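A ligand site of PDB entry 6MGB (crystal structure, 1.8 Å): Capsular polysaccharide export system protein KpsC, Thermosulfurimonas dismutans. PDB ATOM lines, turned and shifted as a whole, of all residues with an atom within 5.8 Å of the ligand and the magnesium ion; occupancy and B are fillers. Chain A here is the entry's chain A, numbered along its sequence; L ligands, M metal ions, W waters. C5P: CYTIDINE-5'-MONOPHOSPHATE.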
ATOM      1  N   SER A 139       9.506  -3.148  22.508  1.00  0.00           N
ATOM      2  CA  SER A 139      10.285  -4.366  22.301  1.00  0.00           C
ATOM      3  C   SER A 139      11.286  -4.100  21.180  1.00  0.00           C
ATOM      4  O   SER A 139      11.528  -2.946  20.807  1.00  0.00           O
ATOM      5  CB  SER A 139       9.351  -5.546  22.012  1.00  0.00           C
ATOM      6  OG  SER A 139       8.585  -5.323  20.835  1.00  0.00           O
ATOM      7  N   LYS A 140      11.880  -5.174  20.646  1.00  0.00           N
ATOM      8  CA  LYS A 140      12.895  -5.021  19.615  1.00  0.00           C
ATOM      9  C   LYS A 140      12.322  -4.416  18.345  1.00  0.00           C
ATOM     10  O   LYS A 140      12.898  -3.477  17.780  1.00  0.00           O
ATOM     11  CB  LYS A 140      13.544  -6.376  19.321  1.00  0.00           C
ATOM     12  CG  LYS A 140      14.798  -6.297  18.449  1.00  0.00           C
ATOM     13  CD  LYS A 140      15.364  -7.678  18.159  1.00  0.00           C
ATOM     14  CE  LYS A 140      16.758  -7.602  17.554  1.00  0.00           C
ATOM     15  NZ  LYS A 140      17.797  -7.289  18.572  1.00  0.00           N
ATOM     16  N   TYR A 141      11.180  -4.932  17.878  1.00  0.00           N
ATOM     17  CA  TYR A 141      10.648  -4.581  16.565  1.00  0.00           C
ATOM     18  C   TYR A 141       9.424  -3.679  16.599  1.00  0.00           C
ATOM     19  O   TYR A 141       9.200  -2.941  15.648  1.00  0.00           O
ATOM     20  CB  TYR A 141      10.310  -5.857  15.775  1.00  0.00           C
ATOM     21  CG  TYR A 141      11.515  -6.735  15.494  1.00  0.00           C
ATOM     22  CD1 TYR A 141      12.555  -6.289  14.683  1.00  0.00           C
ATOM     23  CD2 TYR A 141      11.606  -8.012  16.032  1.00  0.00           C
ATOM     24  CE1 TYR A 141      13.648  -7.091  14.423  1.00  0.00           C
ATOM     25  CE2 TYR A 141      12.693  -8.818  15.780  1.00  0.00           C
ATOM     26  CZ  TYR A 141      13.714  -8.357  14.975  1.00  0.00           C
ATOM     27  OH  TYR A 141      14.808  -9.160  14.715  1.00  0.00           O
ATOM     28  N   LEU A 161       6.002 -21.237  25.306  1.00  0.00           N
ATOM     29  CA  LEU A 161       7.274 -21.649  24.728  1.00  0.00           C
ATOM     30  C   LEU A 161       7.624 -20.684  23.598  1.00  0.00           C
ATOM     31  O   LEU A 161       6.769 -20.389  22.742  1.00  0.00           O
ATOM     32  CB  LEU A 161       7.204 -23.085  24.197  1.00  0.00           C
ATOM     33  CG  LEU A 161       7.333 -24.230  25.211  1.00  0.00           C
ATOM     34  CD1 LEU A 161       6.437 -24.030  26.428  1.00  0.00           C
ATOM     35  CD2 LEU A 161       6.986 -25.546  24.528  1.00  0.00           C
ATOM     36  N   ILE A 162       8.857 -20.200  23.589  1.00  0.00           N
ATOM     37  CA  ILE A 162       9.323 -19.238  22.600  1.00  0.00           C
ATOM     38  C   ILE A 162      10.049 -20.001  21.497  1.00  0.00           C
ATOM     39  O   ILE A 162      11.010 -20.726  21.758  1.00  0.00           O
ATOM     40  CB  ILE A 162      10.239 -18.177  23.223  1.00  0.00           C
ATOM     41  CG1 ILE A 162       9.482 -17.409  24.317  1.00  0.00           C
ATOM     42  CG2 ILE A 162      10.771 -17.220  22.159  1.00  0.00           C
ATOM     43  CD1 ILE A 162      10.343 -16.451  25.117  1.00  0.00           C
ATOM     44  N   ASP A 163       9.591 -19.835  20.256  1.00  0.00           N
ATOM     45  CA  ASP A 163      10.260 -20.421  19.117  1.00  0.00           C
ATOM     46  C   ASP A 163      11.230 -19.403  18.527  1.00  0.00           C
ATOM     47  O   ASP A 163      11.095 -18.196  18.733  1.00  0.00           O
ATOM     48  CB  ASP A 163       9.257 -20.881  18.053  1.00  0.00           C
ATOM     49  CG  ASP A 163       9.858 -21.872  17.066  1.00  0.00           C
ATOM     50  OD1 ASP A 163      10.906 -22.461  17.366  1.00  0.00           O
ATOM     51  OD2 ASP A 163       9.258 -22.065  15.983  1.00  0.00           O
ATOM     52  N   GLN A 164      12.220 -19.905  17.784  1.00  0.00           N
ATOM     53  CA  GLN A 164      13.244 -19.059  17.189  1.00  0.00           C
ATOM     54  C   GLN A 164      13.384 -19.411  15.710  1.00  0.00           C
ATOM     55  O   GLN A 164      12.726 -20.320  15.198  1.00  0.00           O
ATOM     56  CB  GLN A 164      14.578 -19.224  17.934  1.00  0.00           C
ATOM     57  CG  GLN A 164      14.559 -18.569  19.305  1.00  0.00           C
ATOM     58  CD  GLN A 164      15.757 -18.948  20.150  1.00  0.00           C
ATOM     59  OE1 GLN A 164      15.633 -19.636  21.158  1.00  0.00           O
ATOM     60  NE2 GLN A 164      16.935 -18.478  19.741  1.00  0.00           N
ATOM     61  N   THR A 165      14.236 -18.654  15.020  1.00  0.00           N
ATOM     62  CA  THR A 165      14.455 -18.838  13.592  1.00  0.00           C
ATOM     63  C   THR A 165      15.589 -19.824  13.366  1.00  0.00           C
ATOM     64  O   THR A 165      16.621 -19.779  14.039  1.00  0.00           O
ATOM     65  CB  THR A 165      14.789 -17.510  12.916  1.00  0.00           C
ATOM     66  OG1 THR A 165      16.045 -17.021  13.402  1.00  0.00           O
ATOM     67  CG2 THR A 165      13.708 -16.478  13.178  1.00  0.00           C
ATOM     68  N   ASP A 168      19.685 -19.359  13.770  1.00  0.00           N
ATOM     69  CA  ASP A 168      19.988 -18.394  14.812  1.00  0.00           C
ATOM     70  C   ASP A 168      21.287 -18.784  15.525  1.00  0.00           C
ATOM     71  O   ASP A 168      21.318 -19.793  16.233  1.00  0.00           O
ATOM     72  CB  ASP A 168      18.824 -18.304  15.797  1.00  0.00           C
ATOM     73  CG  ASP A 168      18.971 -17.178  16.800  1.00  0.00           C
ATOM     74  OD1 ASP A 168      20.046 -16.562  16.860  1.00  0.00           O
ATOM     75  OD2 ASP A 168      17.983 -16.918  17.518  1.00  0.00           O
ATOM     76  N   SER A 170      22.595 -17.666  18.100  1.00  0.00           N
ATOM     77  CA  SER A 170      22.520 -17.654  19.552  1.00  0.00           C
ATOM     78  C   SER A 170      22.167 -19.017  20.129  1.00  0.00           C
ATOM     79  O   SER A 170      22.330 -19.219  21.344  1.00  0.00           O
ATOM     80  CB  SER A 170      21.500 -16.614  20.015  1.00  0.00           C
ATOM     81  OG  SER A 170      20.173 -17.055  19.770  1.00  0.00           O
ATOM     82  N   LYS A 200       4.849 -19.670  20.649  1.00  0.00           N
ATOM     83  CA  LYS A 200       4.855 -18.422  19.900  1.00  0.00           C
ATOM     84  C   LYS A 200       5.873 -18.529  18.781  1.00  0.00           C
ATOM     85  O   LYS A 200       7.078 -18.633  19.025  1.00  0.00           O
ATOM     86  CB  LYS A 200       5.150 -17.231  20.805  1.00  0.00           C
ATOM     87  CG  LYS A 200       5.259 -15.897  20.068  1.00  0.00           C
ATOM     88  CD  LYS A 200       4.071 -15.669  19.142  1.00  0.00           C
ATOM     89  CE  LYS A 200       4.026 -14.261  18.583  1.00  0.00           C
ATOM     90  NZ  LYS A 200       5.314 -13.866  17.948  1.00  0.00           N
ATOM     91  N   VAL A 201       5.390 -18.503  17.531  1.00  0.00           N
ATOM     92  CA  VAL A 201       6.263 -18.546  16.375  1.00  0.00           C
ATOM     93  C   VAL A 201       6.960 -17.193  16.204  1.00  0.00           C
ATOM     94  O   VAL A 201       6.386 -16.132  16.490  1.00  0.00           O
ATOM     95  CB  VAL A 201       5.470 -18.930  15.117  1.00  0.00           C
ATOM     96  CG1 VAL A 201       6.343 -18.861  13.867  1.00  0.00           C
ATOM     97  CG2 VAL A 201       4.888 -20.333  15.268  1.00  0.00           C
ATOM     98  N   HIS A 202       8.196 -17.243  15.714  1.00  0.00           N
ATOM     99  CA  HIS A 202       8.994 -16.031  15.563  1.00  0.00           C
ATOM    100  C   HIS A 202       8.432 -15.169  14.430  1.00  0.00           C
ATOM    101  O   HIS A 202       8.002 -15.707  13.399  1.00  0.00           O
ATOM    102  CB  HIS A 202      10.448 -16.405  15.279  1.00  0.00           C
ATOM    103  CG  HIS A 202      11.413 -15.271  15.393  1.00  0.00           C
ATOM    104  ND1 HIS A 202      11.531 -14.299  14.427  1.00  0.00           N
ATOM    105  CD2 HIS A 202      12.328 -14.972  16.350  1.00  0.00           C
ATOM    106  CE1 HIS A 202      12.468 -13.439  14.776  1.00  0.00           C
ATOM    107  NE2 HIS A 202      12.967 -13.821  15.939  1.00  0.00           N
ATOM    108  N   PRO A 203       8.426 -13.844  14.577  1.00  0.00           N
ATOM    109  CA  PRO A 203       7.833 -13.002  13.519  1.00  0.00           C
ATOM    110  C   PRO A 203       8.467 -13.198  12.143  1.00  0.00           C
ATOM    111  O   PRO A 203       7.747 -13.145  11.133  1.00  0.00           O
ATOM    112  CB  PRO A 203       8.042 -11.571  14.045  1.00  0.00           C
ATOM    113  CG  PRO A 203       9.062 -11.682  15.132  1.00  0.00           C
ATOM    114  CD  PRO A 203       8.858 -13.036  15.732  1.00  0.00           C
ATOM    115  N   GLU A 204       9.782 -13.398  12.070  1.00  0.00           N
ATOM    116  CA  GLU A 204      10.415 -13.635  10.782  1.00  0.00           C
ATOM    117  C   GLU A 204       9.912 -14.929  10.140  1.00  0.00           C
ATOM    118  O   GLU A 204       9.952 -15.061   8.913  1.00  0.00           O
ATOM    119  CB  GLU A 204      11.934 -13.672  10.933  1.00  0.00           C
ATOM    120  CG  GLU A 204      12.553 -12.316  11.220  1.00  0.00           C
ATOM    121  CD  GLU A 204      14.050 -12.403  11.464  1.00  0.00           C
ATOM    122  OE1 GLU A 204      14.679 -13.357  10.978  1.00  0.00           O
ATOM    123  OE2 GLU A 204      14.590 -11.516  12.160  1.00  0.00           O
ATOM    124  N   PHE A 230       1.273 -10.989  17.449  1.00  0.00           N
ATOM    125  CA  PHE A 230       0.982 -10.261  18.676  1.00  0.00           C
ATOM    126  C   PHE A 230       2.182  -9.472  19.135  1.00  0.00           C
ATOM    127  O   PHE A 230       3.339  -9.873  18.936  1.00  0.00           O
ATOM    128  CB  PHE A 230       0.555 -11.228  19.775  1.00  0.00           C
ATOM    129  CG  PHE A 230      -0.775 -11.875  19.545  1.00  0.00           C
ATOM    130  CD1 PHE A 230      -1.869 -11.125  19.156  1.00  0.00           C
ATOM    131  CD2 PHE A 230      -0.935 -13.238  19.727  1.00  0.00           C
ATOM    132  CE1 PHE A 230      -3.097 -11.719  18.950  1.00  0.00           C
ATOM    133  CE2 PHE A 230      -2.158 -13.845  19.518  1.00  0.00           C
ATOM    134  CZ  PHE A 230      -3.244 -13.083  19.128  1.00  0.00           C
ATOM    135  N   PRO A 232       4.876  -8.769  21.462  1.00  0.00           N
ATOM    136  CA  PRO A 232       5.434  -9.811  22.352  1.00  0.00           C
ATOM    137  C   PRO A 232       5.274  -9.505  23.834  1.00  0.00           C
ATOM    138  O   PRO A 232       5.005 -10.417  24.619  1.00  0.00           O
ATOM    139  CB  PRO A 232       6.913  -9.869  21.935  1.00  0.00           C
ATOM    140  CG  PRO A 232       7.191  -8.559  21.274  1.00  0.00           C
ATOM    141  CD  PRO A 232       5.910  -8.176  20.598  1.00  0.00           C
ATOM    142  N   SER A 246      17.332 -19.546  23.692  1.00  0.00           N
ATOM    143  CA  SER A 246      18.264 -18.417  23.724  1.00  0.00           C
ATOM    144  C   SER A 246      17.669 -17.129  23.159  1.00  0.00           C
ATOM    145  O   SER A 246      18.438 -16.211  22.825  1.00  0.00           O
ATOM    146  CB  SER A 246      19.523 -18.761  22.927  1.00  0.00           C
ATOM    147  OG  SER A 246      19.221 -18.964  21.552  1.00  0.00           O
ATOM    148  N   SER A 247      16.345 -17.016  23.059  1.00  0.00           N
ATOM    149  CA  SER A 247      15.737 -15.862  22.403  1.00  0.00           C
ATOM    150  C   SER A 247      15.850 -14.606  23.270  1.00  0.00           C
ATOM    151  O   SER A 247      15.789 -14.661  24.495  1.00  0.00           O
ATOM    152  CB  SER A 247      14.265 -16.151  22.110  1.00  0.00           C
ATOM    153  OG  SER A 247      13.616 -14.994  21.587  1.00  0.00           O
ATOM    154  N   GLN A 248      15.997 -13.457  22.604  1.00  0.00           N
ATOM    155  CA  GLN A 248      15.928 -12.180  23.302  1.00  0.00           C
ATOM    156  C   GLN A 248      14.579 -11.988  23.981  1.00  0.00           C
ATOM    157  O   GLN A 248      14.474 -11.253  24.961  1.00  0.00           O
ATOM    158  CB  GLN A 248      16.193 -11.025  22.338  1.00  0.00           C
ATOM    159  CG  GLN A 248      16.072  -9.639  22.969  1.00  0.00           C
ATOM    160  CD  GLN A 248      16.316  -8.517  21.971  1.00  0.00           C
ATOM    161  OE1 GLN A 248      16.964  -8.722  20.941  1.00  0.00           O
ATOM    162  NE2 GLN A 248      15.790  -7.339  22.270  1.00  0.00           N
ATOM    163  N   MET A 249      13.541 -12.648  23.467  1.00  0.00           N
ATOM    164  CA  MET A 249      12.222 -12.531  24.077  1.00  0.00           C
ATOM    165  C   MET A 249      12.210 -13.070  25.504  1.00  0.00           C
ATOM    166  O   MET A 249      11.348 -12.689  26.298  1.00  0.00           O
ATOM    167  CB  MET A 249      11.176 -13.250  23.217  1.00  0.00           C
ATOM    168  CG  MET A 249       9.741 -13.042  23.675  1.00  0.00           C
ATOM    169  SD  MET A 249       8.555 -13.571  22.424  1.00  0.00           S
ATOM    170  CE  MET A 249       7.013 -13.360  23.318  1.00  0.00           C
ATOM    171  N   GLU A 252      12.978 -10.064  27.492  1.00  0.00           N
ATOM    172  CA  GLU A 252      11.795  -9.225  27.539  1.00  0.00           C
ATOM    173  C   GLU A 252      10.798  -9.751  28.573  1.00  0.00           C
ATOM    174  O   GLU A 252      10.136  -8.967  29.261  1.00  0.00           O
ATOM    175  CB  GLU A 252      11.162  -9.126  26.158  1.00  0.00           C
ATOM    176  CG  GLU A 252      12.020  -8.362  25.165  1.00  0.00           C
ATOM    177  CD  GLU A 252      11.423  -8.308  23.775  1.00  0.00           C
ATOM    178  OE1 GLU A 252      10.427  -9.008  23.517  1.00  0.00           O
ATOM    179  OE2 GLU A 252      11.963  -7.556  22.940  1.00  0.00           O
HETATM  180  O3P C5P L   1      16.364 -13.310  19.789  1.00  0.00           O
HETATM  181  P   C5P L   1      15.246 -13.503  18.785  1.00  0.00           P
HETATM  182  O1P C5P L   1      14.664 -14.895  18.956  1.00  0.00           O
HETATM  183  O2P C5P L   1      15.551 -13.280  17.315  1.00  0.00           O
HETATM  184  O5' C5P L   1      14.117 -12.460  19.207  1.00  0.00           O
HETATM  185  C5' C5P L   1      14.142 -11.111  18.780  1.00  0.00           C
HETATM  186  C4' C5P L   1      12.893 -10.391  19.218  1.00  0.00           C
HETATM  187  O4' C5P L   1      11.781 -10.836  18.404  1.00  0.00           O
HETATM  188  C3' C5P L   1      12.447 -10.657  20.654  1.00  0.00           C
HETATM  189  O3' C5P L   1      13.112  -9.828  21.591  1.00  0.00           O
HETATM  190  C2' C5P L   1      10.947 -10.421  20.590  1.00  0.00           C
HETATM  191  O2' C5P L   1      10.639  -9.034  20.673  1.00  0.00           O
HETATM  192  C1' C5P L   1      10.609 -10.926  19.184  1.00  0.00           C
HETATM  193  N1  C5P L   1      10.149 -12.331  19.198  1.00  0.00           N
HETATM  194  C2  C5P L   1       8.688 -12.662  19.109  1.00  0.00           C
HETATM  195  N3  C5P L   1       8.239 -14.092  19.117  1.00  0.00           N
HETATM  196  C4  C5P L   1       9.212 -15.174  19.208  1.00  0.00           C
HETATM  197  C5  C5P L   1      10.664 -14.854  19.298  1.00  0.00           C
HETATM  198  C6  C5P L   1      11.117 -13.416  19.296  1.00  0.00           C
HETATM  199  O2  C5P L   1       7.895 -11.780  19.028  1.00  0.00           O
HETATM  200  N4  C5P L   1       8.771 -16.565  19.229  1.00  0.00           N
HETATM  201 MG    MG M   1      16.830 -12.817  15.760  1.00  0.00          MG
HETATM  202  O   HOH W   1       5.282 -11.905  20.142  1.00  0.00           O
HETATM  203  O   HOH W   2       7.799  -9.334  17.286  1.00  0.00           O
HETATM  204  O   HOH W   3      15.345 -16.331  16.722  1.00  0.00           O
HETATM  205  O   HOH W   4      16.121 -14.481  14.722  1.00  0.00           O
HETATM  206  O   HOH W   5      17.681 -10.993  19.290  1.00  0.00           O
HETATM  207  O   HOH W   6      15.248 -11.642  14.846  1.00  0.00           O
HETATM  208  O   HOH W   7      17.527 -10.998  16.651  1.00  0.00           O
HETATM  209  O   HOH W   8       9.660  -7.259  18.840  1.00  0.00           O
HETATM  210  O   HOH W   9      18.436 -14.956  19.323  1.00  0.00           O
HETATM  211  O   HOH W  10      18.491 -13.827  16.506  1.00  0.00           O
HETATM  212  O   HOH W  11      18.126 -12.254  14.202  1.00  0.00           O
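An oxygen (O3') of the ligand is in hydrogen-bond range of the backbone NH (N) of Met 249 (3.4 Å).
An oxygen (O3P) of the ligand lies within hydrogen-bond range of the backbone NH (N) of Gln 248, at 2.8 Å.
OE1 of Glu 252 sits at hydrogen-bond distance from O2' of the ligand (2.9 Å).
O2P of the ligand lies close to NE2 of His 202 (3.0 Å).
The side-chain hydroxyl (OG) of Ser 247 is in hydrogen-bond range of an oxygen (O1P) of the ligand, at 2.8 Å.
A nitrogen (N4) of the ligand sits at hydrogen-bond distance from the backbone carbonyl oxygen (O) of Lys 200 (2.7 Å).
A nitrogen (N4) of the ligand is in hydrogen-bond range of the backbone carbonyl oxygen (O) of Asp 163.
N3 of the ligand is in hydrogen-bond range of NZ of Lys 200, at 3.2 Å.
The side-chain carboxylate (OE2) of Glu 252 lies within hydrogen-bond range of the backbone NH (N) of Lys 140 (3.3 Å).
OG of Ser 247 lies within hydrogen-bond range of N of Met 249, 3.0 Å away.
OH of Tyr 141 lies within hydrogen-bond range of OE2 of Glu 204 (3.5 Å).
The backbone NH (N) of Glu 204 sits at hydrogen-bond distance from a ring nitrogen (ND1) of His 202, 3.1 Å away.
OE1 of Gln 248 is in hydrogen-bond range of NZ of Lys 140 (2.9 Å).
The backbone carbonyl oxygen (O) of Lys 200 lies within hydrogen-bond range of the backbone NH (N) of Asp 163, 3.0 Å away.
The side-chain hydroxyl of Ser 246 sits at hydrogen-bond distance from the side-chain amide nitrogen of Gln 164 (3.0 Å).
O of Leu 161 lies within hydrogen-bond range of N of Lys 200, 2.9 Å away.
Residues that only touch the ligand: Ser 139 (3.95 Å), Lys 140 (3.7 Å), Tyr 141 (3.4 Å), Ile 162 (3.6 Å), Gln 164 (3.7 Å), Val 201 (3.6 Å), Pro 203 (3.4 Å) and Pro 232 (3.5 Å).
Hydrophobic or aromatic side chains that line the ligand: Tyr 141, Ile 162, His 202, Pro 203, Pro 232 and Met 249.
Merely in contact with the magnesium ion: His 202 (3.995 Å).
Of the 22 residues printed, 1 comes within 4 Å of the magnesium ion.
The magnesium ion is bound by O2P of the ligand (2.1 Å), water W10 (2.1 Å), water W4 (2.1 Å), water W11 (2.1 Å), water W7 (2.1 Å) and water W6 (2.2 Å).
Water W6 lies within hydrogen-bond range of OH of Tyr 141, OE2 of Glu 204 and NE2 of His 202.
Water W4 lies within hydrogen-bond range of the side-chain hydroxyl of Thr 165 (2.9 Å) and a ring nitrogen (NE2) of His 202 (3.4 Å).
Water W9 lies within hydrogen-bond range of O3P of the ligand (2.7 Å), OD2 of Asp 168 (2.7 Å) and OG of Ser 170 (2.8 Å).
Water W5 lies within hydrogen-bond range of O3P of the ligand (2.7 Å) and OE1 of Gln 248 (2.9 Å).
Water W8 lies within hydrogen-bond range of O2' of the ligand (2.7 Å), N of Tyr 141 (2.9 Å) and OG of Ser 139 (3.0 Å).
Water W3 lies within hydrogen-bond range of O1P of the ligand, OD2 of Asp 168 and N of Thr 165.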
